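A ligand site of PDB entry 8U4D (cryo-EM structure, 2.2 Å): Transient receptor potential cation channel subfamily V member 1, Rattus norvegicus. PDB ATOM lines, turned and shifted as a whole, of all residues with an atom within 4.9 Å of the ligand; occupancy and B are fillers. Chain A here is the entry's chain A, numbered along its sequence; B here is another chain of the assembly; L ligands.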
ATOM      1  N   ARG A 303      31.747 -24.542  34.714  1.00  0.00           N
ATOM      2  CA  ARG A 303      32.034 -23.271  34.058  1.00  0.00           C
ATOM      3  C   ARG A 303      31.546 -22.084  34.880  1.00  0.00           C
ATOM      4  O   ARG A 303      32.176 -21.028  34.900  1.00  0.00           O
ATOM      5  CB  ARG A 303      31.427 -23.255  32.662  1.00  0.00           C
ATOM      6  CG  ARG A 303      29.912 -23.281  32.624  1.00  0.00           C
ATOM      7  CD  ARG A 303      29.416 -23.375  31.193  1.00  0.00           C
ATOM      8  NE  ARG A 303      30.108 -22.439  30.329  1.00  0.00           N
ATOM      9  CZ  ARG A 303      29.586 -21.325  29.836  1.00  0.00           C
ATOM     10  NH1 ARG A 303      28.335 -20.975  30.074  1.00  0.00           N
ATOM     11  NH2 ARG A 303      30.340 -20.541  29.064  1.00  0.00           N
ATOM     12  N   HIS A 304      30.402 -22.238  35.566  1.00  0.00           N
ATOM     13  CA  HIS A 304      29.869 -21.129  36.352  1.00  0.00           C
ATOM     14  C   HIS A 304      30.538 -21.008  37.715  1.00  0.00           C
ATOM     15  O   HIS A 304      30.403 -19.954  38.358  1.00  0.00           O
ATOM     16  CB  HIS A 304      28.354 -21.284  36.530  1.00  0.00           C
ATOM     17  CG  HIS A 304      27.597 -21.345  35.242  1.00  0.00           C
ATOM     18  ND1 HIS A 304      27.797 -20.446  34.216  1.00  0.00           N
ATOM     19  CD2 HIS A 304      26.646 -22.201  34.809  1.00  0.00           C
ATOM     20  CE1 HIS A 304      27.000 -20.740  33.212  1.00  0.00           C
ATOM     21  NE2 HIS A 304      26.294 -21.801  33.541  1.00  0.00           N
ATOM     22  N   ASP A 403      23.208 -21.619  24.750  1.00  0.00           N
ATOM     23  CA  ASP A 403      23.931 -20.459  25.214  1.00  0.00           C
ATOM     24  C   ASP A 403      23.645 -19.303  24.258  1.00  0.00           C
ATOM     25  O   ASP A 403      22.854 -19.439  23.315  1.00  0.00           O
ATOM     26  CB  ASP A 403      25.431 -20.747  25.304  1.00  0.00           C
ATOM     27  CG  ASP A 403      25.870 -21.209  26.685  1.00  0.00           C
ATOM     28  OD1 ASP A 403      24.999 -21.603  27.498  1.00  0.00           O
ATOM     29  OD2 ASP A 403      27.088 -21.175  26.971  1.00  0.00           O
ATOM     30  N   SER A 404      24.266 -18.163  24.507  1.00  0.00           N
ATOM     31  CA  SER A 404      24.188 -17.025  23.587  1.00  0.00           C
ATOM     32  C   SER A 404      22.748 -16.596  23.322  1.00  0.00           C
ATOM     33  O   SER A 404      22.367 -16.309  22.191  1.00  0.00           O
ATOM     34  CB  SER A 404      24.902 -17.345  22.282  1.00  0.00           C
ATOM     35  OG  SER A 404      24.214 -18.350  21.554  1.00  0.00           O
ATOM     36  N   TYR A 405      21.922 -16.544  24.377  1.00  0.00           N
ATOM     37  CA  TYR A 405      20.555 -16.066  24.219  1.00  0.00           C
ATOM     38  C   TYR A 405      20.523 -14.601  23.802  1.00  0.00           C
ATOM     39  O   TYR A 405      19.800 -14.221  22.880  1.00  0.00           O
ATOM     40  CB  TYR A 405      19.759 -16.276  25.512  1.00  0.00           C
ATOM     41  CG  TYR A 405      19.508 -17.715  25.849  1.00  0.00           C
ATOM     42  CD1 TYR A 405      18.900 -18.569  24.943  1.00  0.00           C
ATOM     43  CD2 TYR A 405      19.863 -18.231  27.095  1.00  0.00           C
ATOM     44  CE1 TYR A 405      18.660 -19.888  25.250  1.00  0.00           C
ATOM     45  CE2 TYR A 405      19.630 -19.554  27.407  1.00  0.00           C
ATOM     46  CZ  TYR A 405      19.027 -20.376  26.482  1.00  0.00           C
ATOM     47  OH  TYR A 405      18.792 -21.686  26.789  1.00  0.00           O
ATOM     48  N   SER A 406      21.315 -13.759  24.482  1.00  0.00           N
ATOM     49  CA  SER A 406      21.250 -12.322  24.221  1.00  0.00           C
ATOM     50  C   SER A 406      21.764 -11.983  22.818  1.00  0.00           C
ATOM     51  O   SER A 406      21.198 -11.108  22.137  1.00  0.00           O
ATOM     52  CB  SER A 406      22.028 -11.556  25.294  1.00  0.00           C
ATOM     53  OG  SER A 406      23.369 -12.008  25.395  1.00  0.00           O
ATOM     54  N   LEU A 409      18.928 -12.809  20.503  1.00  0.00           N
ATOM     55  CA  LEU A 409      17.799 -11.881  20.608  1.00  0.00           C
ATOM     56  C   LEU A 409      18.103 -10.561  19.911  1.00  0.00           C
ATOM     57  O   LEU A 409      17.262 -10.035  19.176  1.00  0.00           O
ATOM     58  CB  LEU A 409      17.451 -11.658  22.083  1.00  0.00           C
ATOM     59  CG  LEU A 409      16.847 -12.886  22.777  1.00  0.00           C
ATOM     60  CD1 LEU A 409      16.796 -12.685  24.279  1.00  0.00           C
ATOM     61  CD2 LEU A 409      15.468 -13.194  22.228  1.00  0.00           C
ATOM     62  N   PHE A 410      19.306 -10.010  20.126  1.00  0.00           N
ATOM     63  CA  PHE A 410      19.662  -8.767  19.445  1.00  0.00           C
ATOM     64  C   PHE A 410      19.735  -8.969  17.933  1.00  0.00           C
ATOM     65  O   PHE A 410      19.290  -8.116  17.159  1.00  0.00           O
ATOM     66  CB  PHE A 410      20.982  -8.228  19.999  1.00  0.00           C
ATOM     67  CG  PHE A 410      20.809  -7.389  21.239  1.00  0.00           C
ATOM     68  CD1 PHE A 410      20.629  -7.988  22.479  1.00  0.00           C
ATOM     69  CD2 PHE A 410      20.823  -6.011  21.180  1.00  0.00           C
ATOM     70  CE1 PHE A 410      20.481  -7.232  23.617  1.00  0.00           C
ATOM     71  CE2 PHE A 410      20.668  -5.250  22.313  1.00  0.00           C
ATOM     72  CZ  PHE A 410      20.492  -5.863  23.536  1.00  0.00           C
ATOM     73  N   PHE A 437       7.262  -5.723  15.630  1.00  0.00           N
ATOM     74  CA  PHE A 437       7.969  -6.830  16.270  1.00  0.00           C
ATOM     75  C   PHE A 437       9.381  -6.412  16.674  1.00  0.00           C
ATOM     76  O   PHE A 437       9.831  -6.705  17.798  1.00  0.00           O
ATOM     77  CB  PHE A 437       8.017  -8.051  15.348  1.00  0.00           C
ATOM     78  CG  PHE A 437       6.712  -8.798  15.268  1.00  0.00           C
ATOM     79  CD1 PHE A 437       5.960  -9.043  16.395  1.00  0.00           C
ATOM     80  CD2 PHE A 437       6.240  -9.253  14.042  1.00  0.00           C
ATOM     81  CE1 PHE A 437       4.761  -9.724  16.316  1.00  0.00           C
ATOM     82  CE2 PHE A 437       5.045  -9.926  13.963  1.00  0.00           C
ATOM     83  CZ  PHE A 437       4.313 -10.171  15.101  1.00  0.00           C
ATOM     84  N   ALA A 440       9.099  -4.141  19.846  1.00  0.00           N
ATOM     85  CA  ALA A 440       8.831  -4.875  21.079  1.00  0.00           C
ATOM     86  C   ALA A 440      10.072  -5.630  21.548  1.00  0.00           C
ATOM     87  O   ALA A 440      10.403  -5.623  22.739  1.00  0.00           O
ATOM     88  CB  ALA A 440       7.649  -5.819  20.878  1.00  0.00           C
ATOM     89  N   MET A 441      10.772  -6.280  20.619  1.00  0.00           N
ATOM     90  CA  MET A 441      11.993  -6.976  21.011  1.00  0.00           C
ATOM     91  C   MET A 441      13.064  -5.993  21.494  1.00  0.00           C
ATOM     92  O   MET A 441      13.794  -6.284  22.439  1.00  0.00           O
ATOM     93  CB  MET A 441      12.537  -7.822  19.856  1.00  0.00           C
ATOM     94  CG  MET A 441      11.714  -9.054  19.585  1.00  0.00           C
ATOM     95  SD  MET A 441      12.422 -10.075  18.289  1.00  0.00           S
ATOM     96  CE  MET A 441      13.883 -10.660  19.156  1.00  0.00           C
ATOM     97  N   THR A 444      12.195  -5.177  25.097  1.00  0.00           N
ATOM     98  CA  THR A 444      12.466  -6.265  26.036  1.00  0.00           C
ATOM     99  C   THR A 444      13.943  -6.587  26.148  1.00  0.00           C
ATOM    100  O   THR A 444      14.368  -7.141  27.172  1.00  0.00           O
ATOM    101  CB  THR A 444      11.682  -7.530  25.665  1.00  0.00           C
ATOM    102  OG1 THR A 444      11.957  -7.908  24.316  1.00  0.00           O
ATOM    103  CG2 THR A 444      10.190  -7.328  25.854  1.00  0.00           C
ATOM    104  N   ASN A 445      14.747  -6.257  25.129  1.00  0.00           N
ATOM    105  CA  ASN A 445      16.184  -6.474  25.175  1.00  0.00           C
ATOM    106  C   ASN A 445      16.901  -5.523  26.123  1.00  0.00           C
ATOM    107  O   ASN A 445      18.092  -5.704  26.366  1.00  0.00           O
ATOM    108  CB  ASN A 445      16.784  -6.347  23.765  1.00  0.00           C
ATOM    109  CG  ASN A 445      16.633  -7.615  22.950  1.00  0.00           C
ATOM    110  OD1 ASN A 445      16.399  -8.697  23.495  1.00  0.00           O
ATOM    111  ND2 ASN A 445      16.769  -7.497  21.645  1.00  0.00           N
ATOM    112  N   LEU A 447      16.522  -5.642  29.123  1.00  0.00           N
ATOM    113  CA  LEU A 447      16.845  -6.485  30.262  1.00  0.00           C
ATOM    114  C   LEU A 447      18.285  -6.980  30.230  1.00  0.00           C
ATOM    115  O   LEU A 447      18.814  -7.387  31.266  1.00  0.00           O
ATOM    116  CB  LEU A 447      15.886  -7.664  30.336  1.00  0.00           C
ATOM    117  CG  LEU A 447      15.860  -8.468  31.651  1.00  0.00           C
ATOM    118  CD1 LEU A 447      15.298  -7.635  32.801  1.00  0.00           C
ATOM    119  CD2 LEU A 447      15.065  -9.740  31.478  1.00  0.00           C
ATOM    120  N   TYR A 448      18.928  -6.948  29.061  1.00  0.00           N
ATOM    121  CA  TYR A 448      20.332  -7.319  28.971  1.00  0.00           C
ATOM    122  C   TYR A 448      21.199  -6.442  29.859  1.00  0.00           C
ATOM    123  O   TYR A 448      22.166  -6.924  30.473  1.00  0.00           O
ATOM    124  CB  TYR A 448      20.809  -7.224  27.517  1.00  0.00           C
ATOM    125  CG  TYR A 448      22.309  -7.268  27.368  1.00  0.00           C
ATOM    126  CD1 TYR A 448      22.995  -8.472  27.259  1.00  0.00           C
ATOM    127  CD2 TYR A 448      23.064  -6.088  27.371  1.00  0.00           C
ATOM    128  CE1 TYR A 448      24.353  -8.515  27.138  1.00  0.00           C
ATOM    129  CE2 TYR A 448      24.422  -6.120  27.259  1.00  0.00           C
ATOM    130  CZ  TYR A 448      25.067  -7.333  27.142  1.00  0.00           C
ATOM    131  OH  TYR A 448      26.429  -7.368  27.022  1.00  0.00           O
ATOM    132  N   ARG A 451      22.436  -6.774  33.849  1.00  0.00           N
ATOM    133  CA  ARG A 451      23.810  -7.143  34.143  1.00  0.00           C
ATOM    134  C   ARG A 451      24.639  -5.866  34.121  1.00  0.00           C
ATOM    135  O   ARG A 451      24.486  -5.031  33.230  1.00  0.00           O
ATOM    136  CB  ARG A 451      24.330  -8.173  33.137  1.00  0.00           C
ATOM    137  CG  ARG A 451      25.024  -7.616  31.907  1.00  0.00           C
ATOM    138  CD  ARG A 451      25.122  -8.644  30.789  1.00  0.00           C
ATOM    139  NE  ARG A 451      23.827  -9.268  30.511  1.00  0.00           N
ATOM    140  CZ  ARG A 451      23.658 -10.448  29.942  1.00  0.00           C
ATOM    141  NH1 ARG A 451      24.670 -11.178  29.537  1.00  0.00           N
ATOM    142  NH2 ARG A 451      22.419 -10.909  29.775  1.00  0.00           N
ATOM    143  N   GLU A 464      15.267 -15.659  33.522  1.00  0.00           N
ATOM    144  CA  GLU A 464      15.652 -16.599  32.474  1.00  0.00           C
ATOM    145  C   GLU A 464      15.423 -18.041  32.931  1.00  0.00           C
ATOM    146  O   GLU A 464      14.871 -18.859  32.185  1.00  0.00           O
ATOM    147  CB  GLU A 464      17.120 -16.392  32.101  1.00  0.00           C
ATOM    148  CG  GLU A 464      17.654 -17.384  31.069  1.00  0.00           C
ATOM    149  CD  GLU A 464      19.083 -17.806  31.337  1.00  0.00           C
ATOM    150  OE1 GLU A 464      19.760 -17.154  32.155  1.00  0.00           O
ATOM    151  OE2 GLU A 464      19.535 -18.790  30.728  1.00  0.00           O
ATOM    152  N   LYS A 465      15.830 -18.355  34.155  1.00  0.00           N
ATOM    153  CA  LYS A 465      15.687 -19.721  34.648  1.00  0.00           C
ATOM    154  C   LYS A 465      14.217 -20.109  34.803  1.00  0.00           C
ATOM    155  O   LYS A 465      13.834 -21.247  34.471  1.00  0.00           O
ATOM    156  CB  LYS A 465      16.438 -19.888  35.967  1.00  0.00           C
ATOM    157  CG  LYS A 465      17.755 -20.647  35.854  1.00  0.00           C
ATOM    158  CD  LYS A 465      18.637 -20.164  34.701  1.00  0.00           C
ATOM    159  CE  LYS A 465      19.850 -21.059  34.526  1.00  0.00           C
ATOM    160  NZ  LYS A 465      20.252 -21.198  33.101  1.00  0.00           N
ATOM    161  N   ILE A 467      11.679 -18.930  33.053  1.00  0.00           N
ATOM    162  CA  ILE A 467      11.190 -19.167  31.704  1.00  0.00           C
ATOM    163  C   ILE A 467      11.615 -20.551  31.226  1.00  0.00           C
ATOM    164  O   ILE A 467      10.797 -21.321  30.698  1.00  0.00           O
ATOM    165  CB  ILE A 467      11.693 -18.075  30.737  1.00  0.00           C
ATOM    166  CG1 ILE A 467      10.921 -16.777  30.947  1.00  0.00           C
ATOM    167  CG2 ILE A 467      11.579 -18.551  29.300  1.00  0.00           C
ATOM    168  CD1 ILE A 467      11.557 -15.568  30.287  1.00  0.00           C
ATOM    169  N   LEU A 468      12.890 -20.896  31.411  1.00  0.00           N
ATOM    170  CA  LEU A 468      13.401 -22.097  30.771  1.00  0.00           C
ATOM    171  C   LEU A 468      12.911 -23.367  31.446  1.00  0.00           C
ATOM    172  O   LEU A 468      12.803 -24.407  30.773  1.00  0.00           O
ATOM    173  CB  LEU A 468      14.932 -22.068  30.734  1.00  0.00           C
ATOM    174  CG  LEU A 468      15.530 -21.054  29.760  1.00  0.00           C
ATOM    175  CD1 LEU A 468      17.044 -21.050  29.840  1.00  0.00           C
ATOM    176  CD2 LEU A 468      15.061 -21.325  28.339  1.00  0.00           C
ATOM    177  N   ILE A 567      25.933 -17.323  37.718  1.00  0.00           N
ATOM    178  CA  ILE A 567      25.665 -17.064  36.315  1.00  0.00           C
ATOM    179  C   ILE A 567      25.782 -15.570  36.017  1.00  0.00           C
ATOM    180  O   ILE A 567      26.322 -15.180  34.978  1.00  0.00           O
ATOM    181  CB  ILE A 567      24.276 -17.610  35.927  1.00  0.00           C
ATOM    182  CG1 ILE A 567      24.304 -19.138  35.843  1.00  0.00           C
ATOM    183  CG2 ILE A 567      23.832 -17.042  34.581  1.00  0.00           C
ATOM    184  CD1 ILE A 567      22.952 -19.779  35.951  1.00  0.00           C
ATOM    185  N   LEU A 570      29.416 -14.732  35.722  1.00  0.00           N
ATOM    186  CA  LEU A 570      29.960 -15.138  34.433  1.00  0.00           C
ATOM    187  C   LEU A 570      29.495 -14.203  33.318  1.00  0.00           C
ATOM    188  O   LEU A 570      30.273 -13.893  32.397  1.00  0.00           O
ATOM    189  CB  LEU A 570      29.574 -16.588  34.135  1.00  0.00           C
ATOM    190  CG  LEU A 570      30.080 -17.133  32.785  1.00  0.00           C
ATOM    191  CD1 LEU A 570      31.593 -17.128  32.734  1.00  0.00           C
ATOM    192  CD2 LEU A 570      29.544 -18.519  32.540  1.00  0.00           C
ATOM    193  N   GLN A 571      28.252 -13.751  33.364  1.00  0.00           N
ATOM    194  CA  GLN A 571      27.761 -12.813  32.364  1.00  0.00           C
ATOM    195  C   GLN A 571      28.555 -11.505  32.396  1.00  0.00           C
ATOM    196  O   GLN A 571      28.931 -10.962  31.351  1.00  0.00           O
ATOM    197  CB  GLN A 571      26.281 -12.515  32.576  1.00  0.00           C
ATOM    198  CG  GLN A 571      25.328 -13.566  32.084  1.00  0.00           C
ATOM    199  CD  GLN A 571      23.894 -13.249  32.456  1.00  0.00           C
ATOM    200  OE1 GLN A 571      23.646 -12.397  33.299  1.00  0.00           O
ATOM    201  NE2 GLN A 571      22.953 -13.936  31.825  1.00  0.00           N
ATOM    202  N   ILE A 574      31.914 -12.044  30.840  1.00  0.00           N
ATOM    203  CA  ILE A 574      31.843 -12.001  29.386  1.00  0.00           C
ATOM    204  C   ILE A 574      31.790 -10.558  28.905  1.00  0.00           C
ATOM    205  O   ILE A 574      32.462 -10.187  27.932  1.00  0.00           O
ATOM    206  CB  ILE A 574      30.626 -12.808  28.888  1.00  0.00           C
ATOM    207  CG1 ILE A 574      30.905 -14.309  28.990  1.00  0.00           C
ATOM    208  CG2 ILE A 574      30.293 -12.453  27.444  1.00  0.00           C
ATOM    209  CD1 ILE A 574      29.663 -15.141  29.170  1.00  0.00           C
ATOM    210  N   PHE B 481       8.552  -3.720  30.285  1.00  0.00           N
ATOM    211  CA  PHE B 481       7.765  -4.575  29.399  1.00  0.00           C
ATOM    212  C   PHE B 481       6.471  -3.905  28.974  1.00  0.00           C
ATOM    213  O   PHE B 481       6.066  -3.973  27.797  1.00  0.00           O
ATOM    214  CB  PHE B 481       7.477  -5.915  30.075  1.00  0.00           C
ATOM    215  CG  PHE B 481       8.652  -6.847  30.114  1.00  0.00           C
ATOM    216  CD1 PHE B 481       9.918  -6.443  29.689  1.00  0.00           C
ATOM    217  CD2 PHE B 481       8.511  -8.132  30.594  1.00  0.00           C
ATOM    218  CE1 PHE B 481      10.979  -7.309  29.729  1.00  0.00           C
ATOM    219  CE2 PHE B 481       9.572  -8.999  30.634  1.00  0.00           C
ATOM    220  CZ  PHE B 481      10.806  -8.588  30.202  1.00  0.00           C
ATOM    221  N   PHE B 485       5.614  -3.018  24.998  1.00  0.00           N
ATOM    222  CA  PHE B 485       4.491  -3.611  24.297  1.00  0.00           C
ATOM    223  C   PHE B 485       3.414  -2.572  23.984  1.00  0.00           C
ATOM    224  O   PHE B 485       2.760  -2.670  22.940  1.00  0.00           O
ATOM    225  CB  PHE B 485       3.914  -4.774  25.104  1.00  0.00           C
ATOM    226  CG  PHE B 485       4.627  -6.073  24.862  1.00  0.00           C
ATOM    227  CD1 PHE B 485       4.360  -6.810  23.728  1.00  0.00           C
ATOM    228  CD2 PHE B 485       5.571  -6.533  25.752  1.00  0.00           C
ATOM    229  CE1 PHE B 485       5.022  -7.997  23.496  1.00  0.00           C
ATOM    230  CE2 PHE B 485       6.233  -7.710  25.528  1.00  0.00           C
ATOM    231  CZ  PHE B 485       5.959  -8.442  24.389  1.00  0.00           C
ATOM    232  N   ILE B 532      -0.755 -11.607  18.582  1.00  0.00           N
ATOM    233  CA  ILE B 532       0.539 -12.138  18.987  1.00  0.00           C
ATOM    234  C   ILE B 532       1.204 -11.202  19.994  1.00  0.00           C
ATOM    235  O   ILE B 532       1.747 -11.663  21.007  1.00  0.00           O
ATOM    236  CB  ILE B 532       1.434 -12.366  17.752  1.00  0.00           C
ATOM    237  CG1 ILE B 532       0.995 -13.631  17.016  1.00  0.00           C
ATOM    238  CG2 ILE B 532       2.897 -12.487  18.160  1.00  0.00           C
ATOM    239  CD1 ILE B 532       1.519 -13.736  15.600  1.00  0.00           C
ATOM    240  N   LEU B 533       1.162  -9.894  19.749  1.00  0.00           N
ATOM    241  CA  LEU B 533       1.726  -8.947  20.698  1.00  0.00           C
ATOM    242  C   LEU B 533       1.018  -9.046  22.052  1.00  0.00           C
ATOM    243  O   LEU B 533       1.675  -9.088  23.093  1.00  0.00           O
ATOM    244  CB  LEU B 533       1.611  -7.524  20.154  1.00  0.00           C
ATOM    245  CG  LEU B 533       2.604  -7.095  19.067  1.00  0.00           C
ATOM    246  CD1 LEU B 533       2.277  -5.691  18.614  1.00  0.00           C
ATOM    247  CD2 LEU B 533       4.046  -7.193  19.562  1.00  0.00           C
ATOM    248  N   ALA B 536       1.963 -12.377  23.817  1.00  0.00           N
ATOM    249  CA  ALA B 536       3.327 -12.326  24.331  1.00  0.00           C
ATOM    250  C   ALA B 536       3.411 -11.462  25.574  1.00  0.00           C
ATOM    251  O   ALA B 536       4.022 -11.858  26.581  1.00  0.00           O
ATOM    252  CB  ALA B 536       4.269 -11.798  23.244  1.00  0.00           C
ATOM    253  N   LEU B 540       4.376 -12.928  29.291  1.00  0.00           N
ATOM    254  CA  LEU B 540       5.574 -12.436  29.957  1.00  0.00           C
ATOM    255  C   LEU B 540       5.237 -11.746  31.284  1.00  0.00           C
ATOM    256  O   LEU B 540       5.963 -11.930  32.265  1.00  0.00           O
ATOM    257  CB  LEU B 540       6.330 -11.479  29.039  1.00  0.00           C
ATOM    258  CG  LEU B 540       7.076 -12.130  27.876  1.00  0.00           C
ATOM    259  CD1 LEU B 540       7.595 -11.071  26.916  1.00  0.00           C
ATOM    260  CD2 LEU B 540       8.221 -13.003  28.364  1.00  0.00           C
HETATM  261  C1  LIG L   1      11.468 -12.657  24.085  1.00  0.00           C
HETATM  262  C2  LIG L   1      11.675 -13.435  25.400  1.00  0.00           C
HETATM  263  C3  LIG L   1      11.850 -12.437  26.570  1.00  0.00           C
HETATM  264  C4  LIG L   1      13.072 -12.839  27.463  1.00  0.00           C
HETATM  265  C5  LIG L   1      13.512 -11.610  28.281  1.00  0.00           C
HETATM  266  C6  LIG L   1      14.589 -10.827  27.497  1.00  0.00           C
HETATM  267  C7  LIG L   1      16.000 -11.424  27.762  1.00  0.00           C
HETATM  268  C8  LIG L   1      17.062 -10.327  27.593  1.00  0.00           C
HETATM  269  C9  LIG L   1      18.401 -10.899  27.070  1.00  0.00           C
HETATM  270  C10 LIG L   1      18.936 -12.756  28.515  1.00  0.00           C
HETATM  271  C11 LIG L   1      18.983 -14.295  28.492  1.00  0.00           C
HETATM  272  C12 LIG L   1      20.262 -14.854  29.122  1.00  0.00           C
HETATM  273  C13 LIG L   1      23.804 -16.691  29.287  1.00  0.00           C
HETATM  274  C14 LIG L   1      25.212 -16.977  29.809  1.00  0.00           C
HETATM  275  C15 LIG L   1      25.453 -18.480  29.998  1.00  0.00           C
HETATM  276  C16 LIG L   1      24.391 -19.099  30.894  1.00  0.00           C
HETATM  277  C17 LIG L   1      22.975 -18.809  30.389  1.00  0.00           C
HETATM  278  C18 LIG L   1       6.914 -12.481  17.796  1.00  0.00           C
HETATM  279  C19 LIG L   1       7.663 -11.628  18.827  1.00  0.00           C
HETATM  280  C20 LIG L   1       6.667 -10.725  19.577  1.00  0.00           C
HETATM  281  C21 LIG L   1       7.234 -10.372  20.968  1.00  0.00           C
HETATM  282  C22 LIG L   1       8.486  -9.477  20.787  1.00  0.00           C
HETATM  283  C23 LIG L   1       8.878  -8.814  22.141  1.00  0.00           C
HETATM  284  O1  LIG L   1      19.158 -10.177  26.530  1.00  0.00           O
HETATM  285  O2  LIG L   1      18.726 -12.288  27.198  1.00  0.00           O
HETATM  286  O3  LIG L   1      21.339 -13.961  28.917  1.00  0.00           O
HETATM  287  O4  LIG L   1      22.494 -15.245  26.978  1.00  0.00           O
HETATM  288  O5  LIG L   1      23.440 -13.350  27.634  1.00  0.00           O
HETATM  289  O6  LIG L   1      23.670 -15.298  29.295  1.00  0.00           O
HETATM  290  P1  LIG L   1      22.731 -14.481  28.194  1.00  0.00           P
HETATM  291  O7  LIG L   1      26.121 -16.466  28.886  1.00  0.00           O
HETATM  292  O8  LIG L   1      17.916 -14.817  29.226  1.00  0.00           O
HETATM  293  O9  LIG L   1      15.788 -14.187  28.961  1.00  0.00           O
HETATM  294  C24 LIG L   1       9.021  -9.842  23.286  1.00  0.00           C
HETATM  295  C25 LIG L   1      10.088 -10.904  22.953  1.00  0.00           C
HETATM  296  C26 LIG L   1      10.155 -11.888  24.126  1.00  0.00           C
HETATM  297  C27 LIG L   1      22.742 -17.322  30.174  1.00  0.00           C
HETATM  298  C28 LIG L   1      16.675 -14.880  28.571  1.00  0.00           C
HETATM  299  C29 LIG L   1      16.437 -15.853  27.395  1.00  0.00           C
HETATM  300  C30 LIG L   1      15.054 -16.500  27.559  1.00  0.00           C
HETATM  301  C31 LIG L   1      14.852 -17.621  26.518  1.00  0.00           C
HETATM  302  C32 LIG L   1      13.876 -17.152  25.433  1.00  0.00           C
HETATM  303  O10 LIG L   1      26.709 -18.656  30.592  1.00  0.00           O
HETATM  304  O11 LIG L   1      22.750 -16.679  31.420  1.00  0.00           O
HETATM  305  O12 LIG L   1      22.055 -19.268  31.349  1.00  0.00           O
HETATM  306  O13 LIG L   1      24.590 -20.484  30.917  1.00  0.00           O
HETATM  307 BR1  LIG L   1       8.658 -13.113  23.981  1.00  0.00          BR
HETATM  308 BR2  LIG L   1      11.416 -13.896  22.607  1.00  0.00          BR
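The backbone NH (N) of Ser 406 is in hydrogen-bond range of an oxygen (O4) of the ligand (3.1 Å). The side-chain hydroxyl (OG) of Ser 406 is in hydrogen-bond range of an oxygen (O5) of the ligand, 2.6 Å away. OE2 of Glu 464 is in hydrogen-bond range of O12 of the ligand (2.6 Å). The side-chain amide nitrogen (NE2) of Gln 571 lies within hydrogen-bond range of an oxygen (O11) of the ligand. The guanidinium group (NH1) of Arg 303 lies within hydrogen-bond range of an oxygen (O10) of the ligand (2.9 Å). N of Tyr 405 lies within hydrogen-bond range of O4 of the ligand. An oxygen (O5) of the ligand is in salt-bridge range of the guanidinium group (NH1) of Arg 451. NZ of Lys 465 is in hydrogen-bond range of O12 of the ligand (3.2 Å). NE2 of His 304 sits close to O13 of the ligand (3.4 Å).
The side-chain carboxylate of Glu 464 lies within salt-bridge range of the side-chain amino group of Lys 465, at 3.5 Å. NH1 of Arg 303 lies within salt-bridge range of OD2 of Asp 403. The backbone carbonyl oxygen of Tyr 448 sits at hydrogen-bond distance from the guanidinium group of Arg 451 (2.9 Å). The backbone carbonyl oxygen (O) of Ala 440 lies within hydrogen-bond range of the side-chain hydroxyl (OG1) of Thr 444, at 3.2 Å. OG1 of Thr 444 lies within hydrogen-bond range of O of Met 441, 3.1 Å away. The side-chain amide nitrogen (ND2) of Asn 445 lies close to the backbone carbonyl oxygen (O) of Met 441.
Residues that only touch the ligand: Ile 567, Leu 570, Ala 440, Met 441, Leu 409, Tyr 448, Phe 485 of chain B, Asp 403, Thr 444, Phe 437, Leu 540 of chain B, Ile 574, Ser 404 and Leu 447. Hydrophobic or aromatic side chains within 4 Å of the ligand: His 304, Tyr 405, Leu 409, Phe 437, Ala 440, Met 441, Leu 447, Tyr 448, Ile 567, Leu 570, Ile 574, Phe 485 of chain B and Leu 540 of chain B. Of the 30 residues printed, 22 come within 4 Å of the ligand. Along chain A the residues within 4 Å of the ligand span positions 303 to 574.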
